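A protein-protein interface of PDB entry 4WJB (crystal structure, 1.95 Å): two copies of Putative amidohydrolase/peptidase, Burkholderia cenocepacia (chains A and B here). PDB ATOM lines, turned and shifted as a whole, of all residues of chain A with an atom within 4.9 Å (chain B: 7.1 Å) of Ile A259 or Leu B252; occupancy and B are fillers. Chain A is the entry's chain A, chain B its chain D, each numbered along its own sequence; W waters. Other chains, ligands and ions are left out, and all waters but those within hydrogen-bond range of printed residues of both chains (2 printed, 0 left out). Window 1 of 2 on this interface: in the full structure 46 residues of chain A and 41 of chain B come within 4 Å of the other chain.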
ATOM      1  N   ALA A 255     -11.770 -18.680  33.576  1.00  0.00           N
ATOM      2  CA  ALA A 255     -12.526 -19.809  33.062  1.00  0.00           C
ATOM      3  C   ALA A 255     -13.429 -19.372  31.914  1.00  0.00           C
ATOM      4  O   ALA A 255     -13.517 -20.056  30.899  1.00  0.00           O
ATOM      5  CB  ALA A 255     -13.343 -20.450  34.170  1.00  0.00           C
ATOM      6  N   ALA A 256     -14.081 -18.222  32.077  1.00  0.00           N
ATOM      7  CA  ALA A 256     -14.951 -17.674  31.039  1.00  0.00           C
ATOM      8  C   ALA A 256     -14.199 -17.506  29.727  1.00  0.00           C
ATOM      9  O   ALA A 256     -14.701 -17.868  28.662  1.00  0.00           O
ATOM     10  CB  ALA A 256     -15.539 -16.345  31.485  1.00  0.00           C
ATOM     11  N   ARG A 257     -12.989 -16.959  29.810  1.00  0.00           N
ATOM     12  CA  ARG A 257     -12.136 -16.809  28.640  1.00  0.00           C
ATOM     13  C   ARG A 257     -11.877 -18.157  27.966  1.00  0.00           C
ATOM     14  O   ARG A 257     -11.900 -18.255  26.741  1.00  0.00           O
ATOM     15  CB  ARG A 257     -10.806 -16.155  29.022  1.00  0.00           C
ATOM     16  CG  ARG A 257     -10.929 -14.733  29.532  1.00  0.00           C
ATOM     17  CD  ARG A 257      -9.571 -14.203  29.988  1.00  0.00           C
ATOM     18  NE  ARG A 257      -9.673 -12.888  30.616  1.00  0.00           N
ATOM     19  CZ  ARG A 257      -9.378 -11.743  30.009  1.00  0.00           C
ATOM     20  NH1 ARG A 257      -8.957 -11.745  28.749  1.00  0.00           N
ATOM     21  NH2 ARG A 257      -9.499 -10.593  30.662  1.00  0.00           N
ATOM     22  N   MET A 258     -11.631 -19.190  28.767  1.00  0.00           N
ATOM     23  CA  MET A 258     -11.331 -20.515  28.231  1.00  0.00           C
ATOM     24  C   MET A 258     -12.571 -21.181  27.634  1.00  0.00           C
ATOM     25  O   MET A 258     -12.485 -21.871  26.618  1.00  0.00           O
ATOM     26  CB  MET A 258     -10.731 -21.415  29.315  1.00  0.00           C
ATOM     27  CG  MET A 258      -9.362 -20.982  29.803  1.00  0.00           C
ATOM     28  SD  MET A 258      -8.173 -20.771  28.466  1.00  0.00           S
ATOM     29  CE  MET A 258      -8.164 -22.410  27.745  1.00  0.00           C
ATOM     30  N   ILE A 259     -13.715 -20.980  28.281  1.00  0.00           N
ATOM     31  CA  ILE A 259     -14.983 -21.529  27.809  1.00  0.00           C
ATOM     32  C   ILE A 259     -15.316 -20.967  26.429  1.00  0.00           C
ATOM     33  O   ILE A 259     -15.708 -21.705  25.518  1.00  0.00           O
ATOM     34  CB  ILE A 259     -16.127 -21.224  28.805  1.00  0.00           C
ATOM     35  CG1 ILE A 259     -15.900 -21.979  30.114  1.00  0.00           C
ATOM     36  CG2 ILE A 259     -17.480 -21.597  28.219  1.00  0.00           C
ATOM     37  CD1 ILE A 259     -16.853 -21.590  31.227  1.00  0.00           C
ATOM     38  N   SER A 260     -15.134 -19.661  26.277  1.00  0.00           N
ATOM     39  CA  SER A 260     -15.365 -18.993  25.002  1.00  0.00           C
ATOM     40  C   SER A 260     -14.393 -19.488  23.943  1.00  0.00           C
ATOM     41  O   SER A 260     -14.761 -19.640  22.770  1.00  0.00           O
ATOM     42  CB  SER A 260     -15.235 -17.473  25.157  1.00  0.00           C
ATOM     43  OG  SER A 260     -16.214 -16.966  26.045  1.00  0.00           O
ATOM     44  N   PHE A 261     -13.152 -19.742  24.355  1.00  0.00           N
ATOM     45  CA  PHE A 261     -12.138 -20.200  23.412  1.00  0.00           C
ATOM     46  C   PHE A 261     -12.409 -21.629  22.959  1.00  0.00           C
ATOM     47  O   PHE A 261     -12.160 -21.975  21.803  1.00  0.00           O
ATOM     48  CB  PHE A 261     -10.736 -20.105  24.013  1.00  0.00           C
ATOM     49  CG  PHE A 261      -9.645 -20.418  23.030  1.00  0.00           C
ATOM     50  CD1 PHE A 261      -9.367 -19.547  21.998  1.00  0.00           C
ATOM     51  CD2 PHE A 261      -8.914 -21.588  23.128  1.00  0.00           C
ATOM     52  CE1 PHE A 261      -8.370 -19.833  21.076  1.00  0.00           C
ATOM     53  CE2 PHE A 261      -7.914 -21.878  22.214  1.00  0.00           C
ATOM     54  CZ  PHE A 261      -7.646 -21.004  21.186  1.00  0.00           C
ATOM     55  N   VAL A 262     -12.910 -22.455  23.873  1.00  0.00           N
ATOM     56  CA  VAL A 262     -13.251 -23.832  23.538  1.00  0.00           C
ATOM     57  C   VAL A 262     -14.297 -23.836  22.429  1.00  0.00           C
ATOM     58  O   VAL A 262     -14.181 -24.592  21.467  1.00  0.00           O
ATOM     59  CB  VAL A 262     -13.766 -24.620  24.766  1.00  0.00           C
ATOM     60  CG1 VAL A 262     -14.431 -25.927  24.330  1.00  0.00           C
ATOM     61  CG2 VAL A 262     -12.619 -24.909  25.726  1.00  0.00           C
ATOM     62  N   GLU A 263     -15.297 -22.965  22.546  1.00  0.00           N
ATOM     63  CA  GLU A 263     -16.291 -22.829  21.488  1.00  0.00           C
ATOM     64  C   GLU A 263     -15.646 -22.399  20.177  1.00  0.00           C
ATOM     65  O   GLU A 263     -15.992 -22.906  19.111  1.00  0.00           O
ATOM     66  CB  GLU A 263     -17.377 -21.826  21.867  1.00  0.00           C
ATOM     67  CG  GLU A 263     -18.454 -21.718  20.791  1.00  0.00           C
ATOM     68  CD  GLU A 263     -19.487 -20.659  21.091  1.00  0.00           C
ATOM     69  OE1 GLU A 263     -20.642 -21.029  21.402  1.00  0.00           O
ATOM     70  OE2 GLU A 263     -19.146 -19.458  21.009  1.00  0.00           O
ATOM     71  N   VAL A 277     -17.399 -27.429  27.118  1.00  0.00           N
ATOM     72  CA  VAL A 277     -17.190 -27.338  28.558  1.00  0.00           C
ATOM     73  C   VAL A 277     -18.539 -27.642  29.198  1.00  0.00           C
ATOM     74  O   VAL A 277     -19.457 -26.829  29.140  1.00  0.00           O
ATOM     75  CB  VAL A 277     -16.660 -25.955  28.987  1.00  0.00           C
ATOM     76  CG1 VAL A 277     -16.563 -25.860  30.511  1.00  0.00           C
ATOM     77  CG2 VAL A 277     -15.301 -25.693  28.355  1.00  0.00           C
ATOM     78  N   ILE A 280     -18.674 -26.993  35.375  1.00  0.00           N
ATOM     79  CA  ILE A 280     -17.884 -25.941  36.003  1.00  0.00           C
ATOM     80  C   ILE A 280     -18.189 -25.867  37.496  1.00  0.00           C
ATOM     81  O   ILE A 280     -19.331 -26.058  37.926  1.00  0.00           O
ATOM     82  CB  ILE A 280     -18.124 -24.555  35.335  1.00  0.00           C
ATOM     83  CG1 ILE A 280     -17.226 -23.480  35.962  1.00  0.00           C
ATOM     84  CG2 ILE A 280     -19.583 -24.151  35.418  1.00  0.00           C
ATOM     85  CD1 ILE A 280     -17.295 -22.144  35.260  1.00  0.00           C
ATOM     86  N   LEU B 233     -29.880 -18.000  32.091  1.00  0.00           N
ATOM     87  CA  LEU B 233     -29.803 -18.289  30.668  1.00  0.00           C
ATOM     88  C   LEU B 233     -30.357 -19.672  30.382  1.00  0.00           C
ATOM     89  O   LEU B 233     -30.034 -20.638  31.075  1.00  0.00           O
ATOM     90  CB  LEU B 233     -28.362 -18.194  30.172  1.00  0.00           C
ATOM     91  CG  LEU B 233     -27.716 -16.812  30.173  1.00  0.00           C
ATOM     92  CD1 LEU B 233     -26.268 -16.931  29.744  1.00  0.00           C
ATOM     93  CD2 LEU B 233     -28.468 -15.855  29.254  1.00  0.00           C
ATOM     94  N   ARG B 249     -27.322 -24.759  21.713  1.00  0.00           N
ATOM     95  CA  ARG B 249     -27.736 -23.615  22.515  1.00  0.00           C
ATOM     96  C   ARG B 249     -27.072 -23.751  23.888  1.00  0.00           C
ATOM     97  O   ARG B 249     -27.690 -24.198  24.851  1.00  0.00           O
ATOM     98  CB  ARG B 249     -29.261 -23.546  22.640  1.00  0.00           C
ATOM     99  CG  ARG B 249     -29.984 -23.357  21.318  1.00  0.00           C
ATOM    100  CD  ARG B 249     -29.680 -22.011  20.691  1.00  0.00           C
ATOM    101  NE  ARG B 249     -30.381 -21.820  19.423  1.00  0.00           N
ATOM    102  CZ  ARG B 249     -29.827 -21.982  18.222  1.00  0.00           C
ATOM    103  NH1 ARG B 249     -28.553 -22.336  18.109  1.00  0.00           N
ATOM    104  NH2 ARG B 249     -30.550 -21.788  17.128  1.00  0.00           N
ATOM    105  N   ASP B 250     -25.793 -23.396  23.948  1.00  0.00           N
ATOM    106  CA  ASP B 250     -24.967 -23.620  25.129  1.00  0.00           C
ATOM    107  C   ASP B 250     -25.070 -22.443  26.103  1.00  0.00           C
ATOM    108  O   ASP B 250     -24.511 -21.379  25.856  1.00  0.00           O
ATOM    109  CB  ASP B 250     -23.511 -23.846  24.695  1.00  0.00           C
ATOM    110  CG  ASP B 250     -22.611 -24.308  25.829  1.00  0.00           C
ATOM    111  OD1 ASP B 250     -22.723 -23.780  26.963  1.00  0.00           O
ATOM    112  OD2 ASP B 250     -21.754 -25.183  25.568  1.00  0.00           O
ATOM    113  N   ALA B 251     -25.775 -22.652  27.211  1.00  0.00           N
ATOM    114  CA  ALA B 251     -26.030 -21.585  28.174  1.00  0.00           C
ATOM    115  C   ALA B 251     -24.774 -21.170  28.936  1.00  0.00           C
ATOM    116  O   ALA B 251     -24.653 -20.027  29.371  1.00  0.00           O
ATOM    117  CB  ALA B 251     -27.123 -22.013  29.156  1.00  0.00           C
ATOM    118  N   LEU B 252     -23.839 -22.099  29.103  1.00  0.00           N
ATOM    119  CA  LEU B 252     -22.614 -21.793  29.831  1.00  0.00           C
ATOM    120  C   LEU B 252     -21.709 -20.857  29.030  1.00  0.00           C
ATOM    121  O   LEU B 252     -21.080 -19.954  29.597  1.00  0.00           O
ATOM    122  CB  LEU B 252     -21.863 -23.079  30.192  1.00  0.00           C
ATOM    123  CG  LEU B 252     -20.569 -22.864  30.983  1.00  0.00           C
ATOM    124  CD1 LEU B 252     -20.814 -21.988  32.222  1.00  0.00           C
ATOM    125  CD2 LEU B 252     -19.944 -24.199  31.380  1.00  0.00           C
ATOM    126  N   VAL B 253     -21.642 -21.070  27.721  1.00  0.00           N
ATOM    127  CA  VAL B 253     -20.887 -20.176  26.844  1.00  0.00           C
ATOM    128  C   VAL B 253     -21.499 -18.777  26.857  1.00  0.00           C
ATOM    129  O   VAL B 253     -20.784 -17.770  26.877  1.00  0.00           O
ATOM    130  CB  VAL B 253     -20.838 -20.697  25.397  1.00  0.00           C
ATOM    131  CG1 VAL B 253     -20.167 -19.674  24.491  1.00  0.00           C
ATOM    132  CG2 VAL B 253     -20.108 -22.035  25.337  1.00  0.00           C
ATOM    133  N   GLY B 254     -22.828 -18.724  26.844  1.00  0.00           N
ATOM    134  CA  GLY B 254     -23.540 -17.466  26.965  1.00  0.00           C
ATOM    135  C   GLY B 254     -23.144 -16.743  28.240  1.00  0.00           C
ATOM    136  O   GLY B 254     -22.875 -15.543  28.223  1.00  0.00           O
ATOM    137  N   ALA B 255     -23.088 -17.485  29.343  1.00  0.00           N
ATOM    138  CA  ALA B 255     -22.717 -16.913  30.633  1.00  0.00           C
ATOM    139  C   ALA B 255     -21.257 -16.459  30.636  1.00  0.00           C
ATOM    140  O   ALA B 255     -20.925 -15.417  31.205  1.00  0.00           O
ATOM    141  CB  ALA B 255     -22.967 -17.918  31.749  1.00  0.00           C
ATOM    142  N   ALA B 256     -20.394 -17.244  29.997  1.00  0.00           N
ATOM    143  CA  ALA B 256     -18.984 -16.903  29.875  1.00  0.00           C
ATOM    144  C   ALA B 256     -18.809 -15.570  29.160  1.00  0.00           C
ATOM    145  O   ALA B 256     -17.976 -14.756  29.546  1.00  0.00           O
ATOM    146  CB  ALA B 256     -18.231 -18.005  29.142  1.00  0.00           C
ATOM    147  N   ARG B 257     -19.605 -15.349  28.121  1.00  0.00           N
ATOM    148  CA  ARG B 257     -19.589 -14.074  27.413  1.00  0.00           C
ATOM    149  C   ARG B 257     -19.965 -12.925  28.349  1.00  0.00           C
ATOM    150  O   ARG B 257     -19.334 -11.864  28.333  1.00  0.00           O
ATOM    151  CB  ARG B 257     -20.542 -14.117  26.221  1.00  0.00           C
ATOM    152  CG  ARG B 257     -20.259 -13.071  25.154  1.00  0.00           C
ATOM    153  CD  ARG B 257     -21.089 -13.343  23.905  1.00  0.00           C
ATOM    154  NE  ARG B 257     -20.303 -13.202  22.683  1.00  0.00           N
ATOM    155  CZ  ARG B 257     -20.576 -13.832  21.544  1.00  0.00           C
ATOM    156  NH1 ARG B 257     -19.805 -13.649  20.480  1.00  0.00           N
ATOM    157  NH2 ARG B 257     -21.618 -14.650  21.467  1.00  0.00           N
ATOM    158  N   MET B 258     -20.991 -13.144  29.167  1.00  0.00           N
ATOM    159  CA  MET B 258     -21.444 -12.124  30.115  1.00  0.00           C
ATOM    160  C   MET B 258     -20.421 -11.876  31.226  1.00  0.00           C
ATOM    161  O   MET B 258     -20.194 -10.732  31.620  1.00  0.00           O
ATOM    162  CB  MET B 258     -22.790 -12.521  30.725  1.00  0.00           C
ATOM    163  CG  MET B 258     -23.944 -12.580  29.731  1.00  0.00           C
ATOM    164  SD  MET B 258     -24.181 -11.030  28.836  1.00  0.00           S
ATOM    165  CE  MET B 258     -24.496  -9.903  30.191  1.00  0.00           C
ATOM    166  N   ILE B 259     -19.817 -12.948  31.734  1.00  0.00           N
ATOM    167  CA  ILE B 259     -18.785 -12.845  32.769  1.00  0.00           C
ATOM    168  C   ILE B 259     -17.608 -11.994  32.293  1.00  0.00           C
ATOM    169  O   ILE B 259     -17.081 -11.158  33.038  1.00  0.00           O
ATOM    170  CB  ILE B 259     -18.274 -14.247  33.194  1.00  0.00           C
ATOM    171  CG1 ILE B 259     -19.359 -14.989  33.978  1.00  0.00           C
ATOM    172  CG2 ILE B 259     -17.013 -14.129  34.040  1.00  0.00           C
ATOM    173  CD1 ILE B 259     -19.123 -16.499  34.108  1.00  0.00           C
ATOM    174  N   ILE B 280     -21.903 -18.841  40.117  1.00  0.00           N
ATOM    175  CA  ILE B 280     -22.419 -19.431  38.889  1.00  0.00           C
ATOM    176  C   ILE B 280     -22.874 -20.868  39.148  1.00  0.00           C
ATOM    177  O   ILE B 280     -22.268 -21.590  39.941  1.00  0.00           O
ATOM    178  CB  ILE B 280     -21.358 -19.394  37.750  1.00  0.00           C
ATOM    179  CG1 ILE B 280     -21.915 -19.989  36.453  1.00  0.00           C
ATOM    180  CG2 ILE B 280     -20.084 -20.103  38.173  1.00  0.00           C
ATOM    181  CD1 ILE B 280     -20.988 -19.832  35.256  1.00  0.00           C
ATOM    182  N   GLU B 281     -23.969 -21.263  38.507  1.00  0.00           N
ATOM    183  CA  GLU B 281     -24.436 -22.640  38.555  1.00  0.00           C
ATOM    184  C   GLU B 281     -24.873 -23.076  37.162  1.00  0.00           C
ATOM    185  O   GLU B 281     -25.809 -22.520  36.602  1.00  0.00           O
ATOM    186  CB  GLU B 281     -25.589 -22.805  39.547  1.00  0.00           C
ATOM    187  CG  GLU B 281     -25.212 -22.530  40.998  1.00  0.00           C
ATOM    188  CD  GLU B 281     -26.244 -23.045  41.981  1.00  0.00           C
ATOM    189  OE1 GLU B 281     -25.991 -22.970  43.202  1.00  0.00           O
ATOM    190  OE2 GLU B 281     -27.307 -23.529  41.535  1.00  0.00           O
ATOM    191  N   ALA B 282     -24.182 -24.062  36.606  1.00  0.00           N
ATOM    192  CA  ALA B 282     -24.553 -24.604  35.300  1.00  0.00           C
ATOM    193  C   ALA B 282     -25.333 -25.898  35.458  1.00  0.00           C
ATOM    194  O   ALA B 282     -25.102 -26.657  36.399  1.00  0.00           O
ATOM    195  CB  ALA B 282     -23.316 -24.834  34.442  1.00  0.00           C
ATOM    196  N   ARG B 283     -26.256 -26.152  34.534  1.00  0.00           N
ATOM    197  CA  ARG B 283     -26.991 -27.409  34.533  1.00  0.00           C
ATOM    198  C   ARG B 283     -27.026 -28.027  33.131  1.00  0.00           C
ATOM    199  O   ARG B 283     -27.072 -27.303  32.134  1.00  0.00           O
ATOM    200  CB  ARG B 283     -28.410 -27.204  35.063  1.00  0.00           C
ATOM    201  CG  ARG B 283     -29.246 -26.231  34.262  1.00  0.00           C
ATOM    202  CD  ARG B 283     -30.727 -26.533  34.432  1.00  0.00           C
ATOM    203  NE  ARG B 283     -31.021 -27.914  34.064  1.00  0.00           N
ATOM    204  CZ  ARG B 283     -31.229 -28.326  32.819  1.00  0.00           C
ATOM    205  NH1 ARG B 283     -31.187 -27.462  31.810  1.00  0.00           N
ATOM    206  NH2 ARG B 283     -31.481 -29.606  32.583  1.00  0.00           N
ATOM    207  N   ASN B 285     -24.552 -29.690  34.246  1.00  0.00           N
ATOM    208  CA  ASN B 285     -23.182 -29.638  34.754  1.00  0.00           C
ATOM    209  C   ASN B 285     -22.485 -30.995  34.652  1.00  0.00           C
ATOM    210  O   ASN B 285     -21.715 -31.372  35.532  1.00  0.00           O
ATOM    211  CB  ASN B 285     -23.158 -29.145  36.208  1.00  0.00           C
ATOM    212  CG  ASN B 285     -21.862 -28.450  36.573  1.00  0.00           C
ATOM    213  OD1 ASN B 285     -21.298 -27.702  35.777  1.00  0.00           O
ATOM    214  ND2 ASN B 285     -21.389 -28.687  37.792  1.00  0.00           N
ATOM    215  N   VAL B 290     -23.802 -30.571  26.615  1.00  0.00           N
ATOM    216  CA  VAL B 290     -23.917 -29.134  26.437  1.00  0.00           C
ATOM    217  C   VAL B 290     -24.851 -28.600  27.512  1.00  0.00           C
ATOM    218  O   VAL B 290     -25.981 -29.068  27.628  1.00  0.00           O
ATOM    219  CB  VAL B 290     -24.454 -28.778  25.040  1.00  0.00           C
ATOM    220  CG1 VAL B 290     -24.470 -27.263  24.844  1.00  0.00           C
ATOM    221  CG2 VAL B 290     -23.608 -29.445  23.961  1.00  0.00           C
ATOM    222  N   PRO B 291     -24.377 -27.640  28.328  1.00  0.00           N
ATOM    223  CA  PRO B 291     -25.236 -27.062  29.367  1.00  0.00           C
ATOM    224  C   PRO B 291     -26.436 -26.335  28.773  1.00  0.00           C
ATOM    225  O   PRO B 291     -26.259 -25.452  27.937  1.00  0.00           O
ATOM    226  CB  PRO B 291     -24.306 -26.079  30.096  1.00  0.00           C
ATOM    227  CG  PRO B 291     -22.933 -26.573  29.812  1.00  0.00           C
ATOM    228  CD  PRO B 291     -22.993 -27.146  28.423  1.00  0.00           C
ATOM    229  N   GLY B 292     -27.637 -26.705  29.203  1.00  0.00           N
ATOM    230  CA  GLY B 292     -28.849 -26.084  28.702  1.00  0.00           C
ATOM    231  C   GLY B 292     -29.376 -25.003  29.627  1.00  0.00           C
ATOM    232  O   GLY B 292     -30.362 -24.336  29.323  1.00  0.00           O
ATOM    233  N   GLY B 293     -28.720 -24.827  30.765  1.00  0.00           N
ATOM    234  CA  GLY B 293     -29.097 -23.767  31.683  1.00  0.00           C
ATOM    235  C   GLY B 293     -27.902 -23.253  32.451  1.00  0.00           C
ATOM    236  O   GLY B 293     -26.948 -23.990  32.710  1.00  0.00           O
ATOM    237  N   CYS B 294     -27.949 -21.978  32.817  1.00  0.00           N
ATOM    238  CA  CYS B 294     -26.906 -21.409  33.642  1.00  0.00           C
ATOM    239  C   CYS B 294     -27.446 -20.212  34.420  1.00  0.00           C
ATOM    240  O   CYS B 294     -28.065 -19.308  33.855  1.00  0.00           O
ATOM    241  CB  CYS B 294     -25.700 -21.005  32.787  1.00  0.00           C
ATOM    242  SG  CYS B 294     -24.240 -20.560  33.774  1.00  0.00           S
ATOM    243  N   LEU B 328     -30.164 -18.061  22.941  1.00  0.00           N
ATOM    244  CA  LEU B 328     -30.484 -18.388  24.328  1.00  0.00           C
ATOM    245  C   LEU B 328     -31.651 -17.552  24.824  1.00  0.00           C
ATOM    246  O   LEU B 328     -31.828 -16.415  24.393  1.00  0.00           O
ATOM    247  CB  LEU B 328     -29.271 -18.161  25.232  1.00  0.00           C
ATOM    248  CG  LEU B 328     -28.061 -19.049  24.960  1.00  0.00           C
ATOM    249  CD1 LEU B 328     -26.851 -18.557  25.727  1.00  0.00           C
ATOM    250  CD2 LEU B 328     -28.372 -20.486  25.321  1.00  0.00           C
HETATM  251  O   HOH W   1     -19.374 -25.191  26.721  1.00  0.00           O
HETATM  252  O   HOH W   2     -21.972 -25.130  38.079  1.00  0.00           O
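Of chain B, only Leu B252 (3.9 Å), Val B253 (3.9 Å) and Ala B256 (3.8 Å) come within 4 Å of Ile A259.
Leu B252 touches just these residues of chain A: Ile A259 (3.9 Å) and Val A277 (3.5 Å).
Of the printed residues of chain B, Ile A280 touches Ala B282 and Asn B285.
Of the printed residues of chain A, Ala B256 touches Ala A256, Ile A259 and Ser A260.
Of the printed residues of chain B, Glu A263 touches Val B253 (3.4 Å).
Printed residues of chain B within 4 Å of Ala A256: Ala B256 and Ile B259.
Arg A257 touches none of the printed residues of chain B.
Asp B250 touches none of the printed residues of chain A.
The nearest printed residue of chain B that does not touch Ile A280 is Leu B252 (4.1 Å).
Of the 23 printed residues of chain B, 7 touch a printed residue of chain A.
Printed residues of chain B that touch a printed residue of chain A: Leu B252, Val B253, Ala B256, Ile B259, Ala B282, Asn B285 and Pro B291.
Printed residues of chain A that touch a printed residue of chain B: Ala A256, Ile A259, Ser A260, Glu A263, Val A277 and Ile A280.
Among the printed residues, 11 pairs touch across the chains.
Water W1 bridges the side-chain carboxylate of Asp B250 (2.6 Å) and the backbone carbonyl oxygen of Val A277 (2.9 Å).
Water W2 lies within hydrogen-bond range of the backbone carbonyl oxygen (O) of Ile A280 (2.8 Å) and the backbone NH (N) of Ala B282 (2.9 Å).
The backbone NH of Val B253 is in hydrogen-bond range of the side-chain carboxylate of Asp B250 (3.0 Å).
O of Ala A256 sits at hydrogen-bond distance from OG of Ser A260 (3.2 Å).
The side-chain carboxylate (OD1) of Asp B250 sits at hydrogen-bond distance from the backbone NH (N) of Leu B252 (2.9 Å).
N of Ala B251 lies within hydrogen-bond range of O of Pro B291 (2.9 Å).
Ala B256 touches its own counterpart, Ala A256.
Ala A256 touches Ile B259, and with the chains exchanged Ile A259 touches Ala B256.
The side-chain amide oxygen (OD1) of Asn B285 is in hydrogen-bond range of the backbone NH (N) of Ile A280 (2.7 Å).
Among the printed residues, pairs that only touch across the chains: Ala A256 with Ala B256, Ala A256 with Ile B259, Ile A259 with Leu B252, Ile A259 with Val B253, Ile A259 with Ala B256, Ser A260 with Ala B256, Glu A263 with Val B253, Val A277 with Leu B252, Val A277 with Pro B291 and Ile A280 with Ala B282.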
